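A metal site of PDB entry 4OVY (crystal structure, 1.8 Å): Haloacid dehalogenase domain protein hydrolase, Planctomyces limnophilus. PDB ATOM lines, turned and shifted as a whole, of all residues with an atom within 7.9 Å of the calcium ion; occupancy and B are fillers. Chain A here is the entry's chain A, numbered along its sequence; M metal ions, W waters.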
ATOM      1  N   ASP A  42      16.861 -16.235 -10.895  1.00  0.00           N
ATOM      2  CA  ASP A  42      18.044 -15.993 -10.078  1.00  0.00           C
ATOM      3  C   ASP A  42      18.119 -14.487  -9.794  1.00  0.00           C
ATOM      4  O   ASP A  42      17.472 -13.682 -10.486  1.00  0.00           O
ATOM      5  CB  ASP A  42      19.296 -16.470 -10.815  1.00  0.00           C
ATOM      6  CG  ASP A  42      20.497 -16.628  -9.887  1.00  0.00           C
ATOM      7  OD1 ASP A  42      20.384 -16.510  -8.659  1.00  0.00           O
ATOM      8  OD2 ASP A  42      21.571 -16.896 -10.422  1.00  0.00           O
ATOM      9  N   ASN A  43      18.888 -14.105  -8.785  1.00  0.00           N
ATOM     10  CA  ASN A  43      19.088 -12.694  -8.458  1.00  0.00           C
ATOM     11  C   ASN A  43      20.431 -12.167  -8.987  1.00  0.00           C
ATOM     12  O   ASN A  43      20.460 -11.429  -9.968  1.00  0.00           O
ATOM     13  CB  ASN A  43      18.980 -12.479  -6.937  1.00  0.00           C
ATOM     14  CG  ASN A  43      19.028 -11.001  -6.553  1.00  0.00           C
ATOM     15  OD1 ASN A  43      18.523 -10.139  -7.285  1.00  0.00           O
ATOM     16  ND2 ASN A  43      19.614 -10.703  -5.403  1.00  0.00           N
ATOM     17  N   ASP A  44      21.530 -12.574  -8.353  1.00  0.00           N
ATOM     18  CA  ASP A  44      22.866 -12.122  -8.758  1.00  0.00           C
ATOM     19  C   ASP A  44      23.101 -12.403 -10.247  1.00  0.00           C
ATOM     20  O   ASP A  44      23.014 -13.540 -10.669  1.00  0.00           O
ATOM     21  CB  ASP A  44      23.951 -12.855  -7.955  1.00  0.00           C
ATOM     22  CG  ASP A  44      23.894 -12.562  -6.460  1.00  0.00           C
ATOM     23  OD1 ASP A  44      23.434 -11.471  -6.049  1.00  0.00           O
ATOM     24  OD2 ASP A  44      24.322 -13.443  -5.696  1.00  0.00           O
ATOM     25  N   GLY A  45      23.387 -11.362 -11.023  1.00  0.00           N
ATOM     26  CA  GLY A  45      23.713 -11.515 -12.439  1.00  0.00           C
ATOM     27  C   GLY A  45      22.515 -11.693 -13.357  1.00  0.00           C
ATOM     28  O   GLY A  45      22.665 -11.742 -14.577  1.00  0.00           O
ATOM     29  N   THR A  46      21.316 -11.799 -12.774  1.00  0.00           N
ATOM     30  CA  THR A  46      20.086 -11.995 -13.522  1.00  0.00           C
ATOM     31  C   THR A  46      19.171 -10.769 -13.359  1.00  0.00           C
ATOM     32  O   THR A  46      18.669 -10.245 -14.347  1.00  0.00           O
ATOM     33  CB  THR A  46      19.386 -13.288 -13.072  1.00  0.00           C
ATOM     34  OG1 THR A  46      20.185 -14.419 -13.459  1.00  0.00           O
ATOM     35  CG2 THR A  46      17.999 -13.426 -13.693  1.00  0.00           C
ATOM     36  N   LEU A  47      18.957 -10.345 -12.112  1.00  0.00           N
ATOM     37  CA  LEU A  47      18.158  -9.161 -11.794  1.00  0.00           C
ATOM     38  C   LEU A  47      19.017  -7.933 -11.459  1.00  0.00           C
ATOM     39  O   LEU A  47      18.552  -6.802 -11.577  1.00  0.00           O
ATOM     40  CB  LEU A  47      17.222  -9.451 -10.619  1.00  0.00           C
ATOM     41  CG  LEU A  47      16.139 -10.503 -10.839  1.00  0.00           C
ATOM     42  CD1 LEU A  47      15.280 -10.682  -9.590  1.00  0.00           C
ATOM     43  CD2 LEU A  47      15.250 -10.139 -12.024  1.00  0.00           C
ATOM     44  N   TRP A  48      20.238  -8.164 -10.998  1.00  0.00           N
ATOM     45  CA  TRP A  48      21.142  -7.076 -10.645  1.00  0.00           C
ATOM     46  C   TRP A  48      22.611  -7.470 -10.795  1.00  0.00           C
ATOM     47  O   TRP A  48      22.924  -8.634 -11.039  1.00  0.00           O
ATOM     48  CB  TRP A  48      20.837  -6.553  -9.229  1.00  0.00           C
ATOM     49  CG  TRP A  48      21.296  -7.408  -8.079  1.00  0.00           C
ATOM     50  CD1 TRP A  48      21.652  -8.729  -8.111  1.00  0.00           C
ATOM     51  CD2 TRP A  48      21.417  -6.995  -6.714  1.00  0.00           C
ATOM     52  NE1 TRP A  48      21.988  -9.151  -6.850  1.00  0.00           N
ATOM     53  CE2 TRP A  48      21.857  -8.110  -5.983  1.00  0.00           C
ATOM     54  CE3 TRP A  48      21.194  -5.793  -6.045  1.00  0.00           C
ATOM     55  CZ2 TRP A  48      22.078  -8.053  -4.610  1.00  0.00           C
ATOM     56  CZ3 TRP A  48      21.430  -5.743  -4.680  1.00  0.00           C
ATOM     57  CH2 TRP A  48      21.868  -6.865  -3.981  1.00  0.00           C
ATOM     58  N   GLU A  50      26.540  -8.382 -10.324  1.00  0.00           N
ATOM     59  CA  GLU A  50      27.316  -9.286  -9.458  1.00  0.00           C
ATOM     60  C   GLU A  50      28.838  -9.135  -9.660  1.00  0.00           C
ATOM     61  O   GLU A  50      29.610 -10.014  -9.274  1.00  0.00           O
ATOM     62  CB  GLU A  50      26.918 -10.738  -9.703  1.00  0.00           C
ATOM     63  CG  GLU A  50      27.240 -11.232 -11.105  1.00  0.00           C
ATOM     64  CD  GLU A  50      26.793 -12.639 -11.396  1.00  0.00           C
ATOM     65  OE1 GLU A  50      26.451 -13.379 -10.447  1.00  0.00           O
ATOM     66  OE2 GLU A  50      26.784 -12.999 -12.591  1.00  0.00           O
ATOM     67  N   TYR A  54      29.755 -10.840  -5.805  1.00  0.00           N
ATOM     68  CA  TYR A  54      28.383 -10.963  -5.315  1.00  0.00           C
ATOM     69  C   TYR A  54      28.187  -9.890  -4.251  1.00  0.00           C
ATOM     70  O   TYR A  54      29.080  -9.678  -3.420  1.00  0.00           O
ATOM     71  CB  TYR A  54      28.108 -12.362  -4.740  1.00  0.00           C
ATOM     72  CG  TYR A  54      28.382 -13.517  -5.691  1.00  0.00           C
ATOM     73  CD1 TYR A  54      27.882 -13.497  -6.995  1.00  0.00           C
ATOM     74  CD2 TYR A  54      29.124 -14.626  -5.288  1.00  0.00           C
ATOM     75  CE1 TYR A  54      28.119 -14.548  -7.861  1.00  0.00           C
ATOM     76  CE2 TYR A  54      29.361 -15.683  -6.161  1.00  0.00           C
ATOM     77  CZ  TYR A  54      28.855 -15.638  -7.446  1.00  0.00           C
ATOM     78  OH  TYR A  54      29.093 -16.673  -8.337  1.00  0.00           O
ATOM     79  N   VAL A 160      14.908 -17.363  -6.857  1.00  0.00           N
ATOM     80  CA  VAL A 160      15.538 -18.631  -6.487  1.00  0.00           C
ATOM     81  C   VAL A 160      17.049 -18.425  -6.642  1.00  0.00           C
ATOM     82  O   VAL A 160      17.597 -18.550  -7.722  1.00  0.00           O
ATOM     83  CB  VAL A 160      15.029 -19.806  -7.329  1.00  0.00           C
ATOM     84  CG1 VAL A 160      15.624 -21.125  -6.853  1.00  0.00           C
ATOM     85  CG2 VAL A 160      13.498 -19.883  -7.274  1.00  0.00           C
ATOM     86  N   SER A 161      17.706 -18.096  -5.521  1.00  0.00           N
ATOM     87  CA  SER A 161      19.095 -17.635  -5.528  1.00  0.00           C
ATOM     88  C   SER A 161      19.961 -18.463  -4.586  1.00  0.00           C
ATOM     89  O   SER A 161      19.478 -19.012  -3.615  1.00  0.00           O
ATOM     90  CB  SER A 161      19.158 -16.163  -5.127  1.00  0.00           C
ATOM     91  OG  SER A 161      20.476 -15.723  -4.831  1.00  0.00           O
ATOM     92  N   GLY A 162      21.252 -18.547  -4.896  1.00  0.00           N
ATOM     93  CA  GLY A 162      22.216 -19.161  -3.990  1.00  0.00           C
ATOM     94  C   GLY A 162      22.575 -18.275  -2.821  1.00  0.00           C
ATOM     95  O   GLY A 162      23.108 -18.747  -1.812  1.00  0.00           O
ATOM     96  N   ASP A 212      21.685 -23.695  -4.596  1.00  0.00           N
ATOM     97  CA  ASP A 212      22.431 -23.505  -5.834  1.00  0.00           C
ATOM     98  C   ASP A 212      22.613 -24.825  -6.573  1.00  0.00           C
ATOM     99  O   ASP A 212      22.527 -25.905  -5.968  1.00  0.00           O
ATOM    100  CB  ASP A 212      23.785 -22.870  -5.542  1.00  0.00           C
ATOM    101  CG  ASP A 212      24.402 -22.154  -6.768  1.00  0.00           C
ATOM    102  OD1 ASP A 212      23.697 -21.920  -7.771  1.00  0.00           O
ATOM    103  OD2 ASP A 212      25.604 -21.833  -6.704  1.00  0.00           O
ATOM    104  N   LYS A 216      18.650 -26.004  -6.586  1.00  0.00           N
ATOM    105  CA  LYS A 216      17.568 -25.092  -6.982  1.00  0.00           C
ATOM    106  C   LYS A 216      16.240 -25.808  -7.262  1.00  0.00           C
ATOM    107  O   LYS A 216      15.199 -25.380  -6.753  1.00  0.00           O
ATOM    108  CB  LYS A 216      17.989 -24.151  -8.120  1.00  0.00           C
ATOM    109  CG  LYS A 216      19.035 -23.121  -7.678  1.00  0.00           C
ATOM    110  CD  LYS A 216      19.173 -21.934  -8.626  1.00  0.00           C
ATOM    111  CE  LYS A 216      20.185 -20.937  -8.078  1.00  0.00           C
ATOM    112  NZ  LYS A 216      20.129 -19.632  -8.777  1.00  0.00           N
ATOM    113  N   VAL A 232      14.445 -17.753 -15.461  1.00  0.00           N
ATOM    114  CA  VAL A 232      15.515 -16.933 -15.990  1.00  0.00           C
ATOM    115  C   VAL A 232      16.718 -16.998 -15.058  1.00  0.00           C
ATOM    116  O   VAL A 232      16.608 -16.806 -13.851  1.00  0.00           O
ATOM    117  CB  VAL A 232      15.088 -15.460 -16.176  1.00  0.00           C
ATOM    118  CG1 VAL A 232      16.172 -14.693 -16.919  1.00  0.00           C
ATOM    119  CG2 VAL A 232      13.749 -15.373 -16.900  1.00  0.00           C
ATOM    120  N   GLY A 233      17.875 -17.273 -15.644  1.00  0.00           N
ATOM    121  CA  GLY A 233      19.131 -17.333 -14.911  1.00  0.00           C
ATOM    122  C   GLY A 233      20.223 -16.681 -15.730  1.00  0.00           C
ATOM    123  O   GLY A 233      19.944 -16.027 -16.743  1.00  0.00           O
ATOM    124  N   ASN A 234      21.475 -16.838 -15.290  1.00  0.00           N
ATOM    125  CA  ASN A 234      22.614 -16.293 -16.026  1.00  0.00           C
ATOM    126  C   ASN A 234      23.904 -17.107 -15.936  1.00  0.00           C
ATOM    127  O   ASN A 234      24.866 -16.802 -16.638  1.00  0.00           O
ATOM    128  CB  ASN A 234      22.925 -14.872 -15.560  1.00  0.00           C
ATOM    129  CG  ASN A 234      23.556 -14.852 -14.180  1.00  0.00           C
ATOM    130  OD1 ASN A 234      22.916 -15.227 -13.209  1.00  0.00           O
ATOM    131  ND2 ASN A 234      24.812 -14.433 -14.094  1.00  0.00           N
ATOM    132  N   SER A 235      23.955 -18.108 -15.069  1.00  0.00           N
ATOM    133  CA  SER A 235      25.210 -18.820 -14.828  1.00  0.00           C
ATOM    134  C   SER A 235      25.008 -20.323 -14.827  1.00  0.00           C
ATOM    135  O   SER A 235      23.878 -20.824 -14.854  1.00  0.00           O
ATOM    136  CB  SER A 235      25.820 -18.352 -13.509  1.00  0.00           C
ATOM    137  OG  SER A 235      25.147 -18.968 -12.409  1.00  0.00           O
ATOM    138  N   ASP A 236      26.108 -21.053 -14.781  1.00  0.00           N
ATOM    139  CA  ASP A 236      26.044 -22.511 -14.733  1.00  0.00           C
ATOM    140  C   ASP A 236      25.364 -23.038 -13.475  1.00  0.00           C
ATOM    141  O   ASP A 236      24.829 -24.137 -13.482  1.00  0.00           O
ATOM    142  CB  ASP A 236      27.433 -23.107 -14.911  1.00  0.00           C
ATOM    143  CG  ASP A 236      27.938 -23.007 -16.346  1.00  0.00           C
ATOM    144  OD1 ASP A 236      27.219 -22.458 -17.227  1.00  0.00           O
ATOM    145  OD2 ASP A 236      29.068 -23.481 -16.593  1.00  0.00           O
ATOM    146  N   GLY A 237      25.378 -22.249 -12.389  1.00  0.00           N
ATOM    147  CA  GLY A 237      24.604 -22.574 -11.196  1.00  0.00           C
ATOM    148  C   GLY A 237      23.090 -22.608 -11.394  1.00  0.00           C
ATOM    149  O   GLY A 237      22.378 -23.144 -10.547  1.00  0.00           O
ATOM    150  N   ASP A 238      22.613 -22.070 -12.522  1.00  0.00           N
ATOM    151  CA  ASP A 238      21.194 -22.094 -12.886  1.00  0.00           C
ATOM    152  C   ASP A 238      20.804 -23.243 -13.819  1.00  0.00           C
ATOM    153  O   ASP A 238      19.629 -23.373 -14.188  1.00  0.00           O
ATOM    154  CB  ASP A 238      20.827 -20.771 -13.569  1.00  0.00           C
ATOM    155  CG  ASP A 238      20.950 -19.584 -12.639  1.00  0.00           C
ATOM    156  OD1 ASP A 238      20.374 -19.665 -11.535  1.00  0.00           O
ATOM    157  OD2 ASP A 238      21.606 -18.597 -13.010  1.00  0.00           O
ATOM    158  N   HIS A 259      26.147 -11.629 -20.218  1.00  0.00           N
ATOM    159  CA  HIS A 259      26.814 -10.358 -19.958  1.00  0.00           C
ATOM    160  C   HIS A 259      27.873 -10.071 -21.010  1.00  0.00           C
ATOM    161  O   HIS A 259      29.029 -10.491 -20.892  1.00  0.00           O
ATOM    162  CB  HIS A 259      27.416 -10.383 -18.567  1.00  0.00           C
ATOM    163  CG  HIS A 259      26.394 -10.451 -17.488  1.00  0.00           C
ATOM    164  ND1 HIS A 259      26.027  -9.361 -16.735  1.00  0.00           N
ATOM    165  CD2 HIS A 259      25.597 -11.477 -17.078  1.00  0.00           C
ATOM    166  CE1 HIS A 259      25.082  -9.710 -15.884  1.00  0.00           C
ATOM    167  NE2 HIS A 259      24.798 -10.983 -16.073  1.00  0.00           N
ATOM    168  N   TYR A 268      31.467 -10.759 -19.318  1.00  0.00           N
ATOM    169  CA  TYR A 268      32.054 -11.975 -18.757  1.00  0.00           C
ATOM    170  C   TYR A 268      31.203 -13.196 -19.072  1.00  0.00           C
ATOM    171  O   TYR A 268      30.000 -13.076 -19.217  1.00  0.00           O
ATOM    172  CB  TYR A 268      32.217 -11.868 -17.242  1.00  0.00           C
ATOM    173  CG  TYR A 268      30.929 -11.659 -16.456  1.00  0.00           C
ATOM    174  CD1 TYR A 268      30.420 -10.392 -16.245  1.00  0.00           C
ATOM    175  CD2 TYR A 268      30.239 -12.751 -15.912  1.00  0.00           C
ATOM    176  CE1 TYR A 268      29.257 -10.197 -15.520  1.00  0.00           C
ATOM    177  CE2 TYR A 268      29.075 -12.573 -15.185  1.00  0.00           C
ATOM    178  CZ  TYR A 268      28.595 -11.296 -14.984  1.00  0.00           C
ATOM    179  OH  TYR A 268      27.438 -11.112 -14.262  1.00  0.00           O
ATOM    180  N   PHE A 274      32.877 -14.991 -10.731  1.00  0.00           N
ATOM    181  CA  PHE A 274      31.526 -14.711 -10.266  1.00  0.00           C
ATOM    182  C   PHE A 274      30.543 -14.822 -11.427  1.00  0.00           C
ATOM    183  O   PHE A 274      30.738 -14.180 -12.457  1.00  0.00           O
ATOM    184  CB  PHE A 274      31.472 -13.314  -9.633  1.00  0.00           C
ATOM    185  CG  PHE A 274      32.399 -13.160  -8.465  1.00  0.00           C
ATOM    186  CD1 PHE A 274      32.072 -13.711  -7.231  1.00  0.00           C
ATOM    187  CD2 PHE A 274      33.602 -12.484  -8.580  1.00  0.00           C
ATOM    188  CE1 PHE A 274      32.912 -13.581  -6.141  1.00  0.00           C
ATOM    189  CE2 PHE A 274      34.457 -12.348  -7.482  1.00  0.00           C
ATOM    190  CZ  PHE A 274      34.108 -12.906  -6.269  1.00  0.00           C
ATOM    191  N   GLY A 275      29.513 -15.641 -11.272  1.00  0.00           N
ATOM    192  CA  GLY A 275      28.517 -15.827 -12.322  1.00  0.00           C
ATOM    193  C   GLY A 275      29.055 -16.498 -13.569  1.00  0.00           C
ATOM    194  O   GLY A 275      28.663 -16.148 -14.693  1.00  0.00           O
ATOM    195  N   ARG A 276      29.946 -17.467 -13.386  1.00  0.00           N
ATOM    196  CA  ARG A 276      30.520 -18.197 -14.511  1.00  0.00           C
ATOM    197  C   ARG A 276      29.435 -18.837 -15.350  1.00  0.00           C
ATOM    198  O   ARG A 276      28.560 -19.537 -14.838  1.00  0.00           O
ATOM    199  CB  ARG A 276      31.506 -19.286 -14.034  1.00  0.00           C
ATOM    200  CG  ARG A 276      32.341 -19.863 -15.167  1.00  0.00           C
ATOM    201  CD  ARG A 276      33.226 -21.007 -14.692  1.00  0.00           C
ATOM    202  NE  ARG A 276      34.054 -20.642 -13.545  1.00  0.00           N
ATOM    203  CZ  ARG A 276      35.242 -20.043 -13.598  1.00  0.00           C
ATOM    204  NH1 ARG A 276      35.797 -19.716 -14.756  1.00  0.00           N
ATOM    205  NH2 ARG A 276      35.882 -19.766 -12.473  1.00  0.00           N
HETATM  206 CA    CA M   1      23.587 -15.908 -10.982  1.00  0.00          CA
HETATM  207  O   HOH W   1      25.586 -15.874 -10.377  1.00  0.00           O
HETATM  208  O   HOH W   2      23.398 -18.700 -10.637  1.00  0.00           O
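Water W2 lies within hydrogen-bond range of OG of Ser 235 (2.5 Å) and OD2 of Asp 238 (3.0 Å).
The calcium ion is bound by water W1 (2.1 Å), OD2 of Asp 42 (2.3 Å), OD1 of Asn 234 (2.4 Å), O of Asp 44 (2.5 Å) and water W2 (2.8 Å).
The calcium ion has five donor atoms within binding distance.
Glu 50 touches the calcium ion (OE1 to CA, 3.9 Å).
Ser 235 touches the calcium ion.
Asp 238 touches the calcium ion (OD2 to CA, 3.9 Å).
Of the 26 residues printed, 6 come within 4 Å of the calcium ion.
The nearest printed residue that does not touch the calcium ion is Thr 46 (4.5 Å).
ND2 of Asn 234 lies within hydrogen-bond range of OE2 of Glu 50 (2.9 Å).
The side-chain amide nitrogen of Asn 234 lies close to the backbone carbonyl oxygen of Gly 45, 3.5 Å away.
OG of Ser 235 lies close to N of Gly 237.
N of Asp 42 lies within hydrogen-bond range of O of Val 232 (3.0 Å).
The side-chain carboxylate of Asp 42 lies within salt-bridge range of the side-chain amino group of Lys 216.
The side-chain carboxylate of Asp 44 is in hydrogen-bond range of the indole nitrogen of Trp 48.
The side-chain hydroxyl (OH) of Tyr 268 is in hydrogen-bond range of the side-chain carboxylate (OE2) of Glu 50, at 2.6 Å.
N of Ser 235 sits at hydrogen-bond distance from OD2 of Asp 238, at 3.2 Å.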
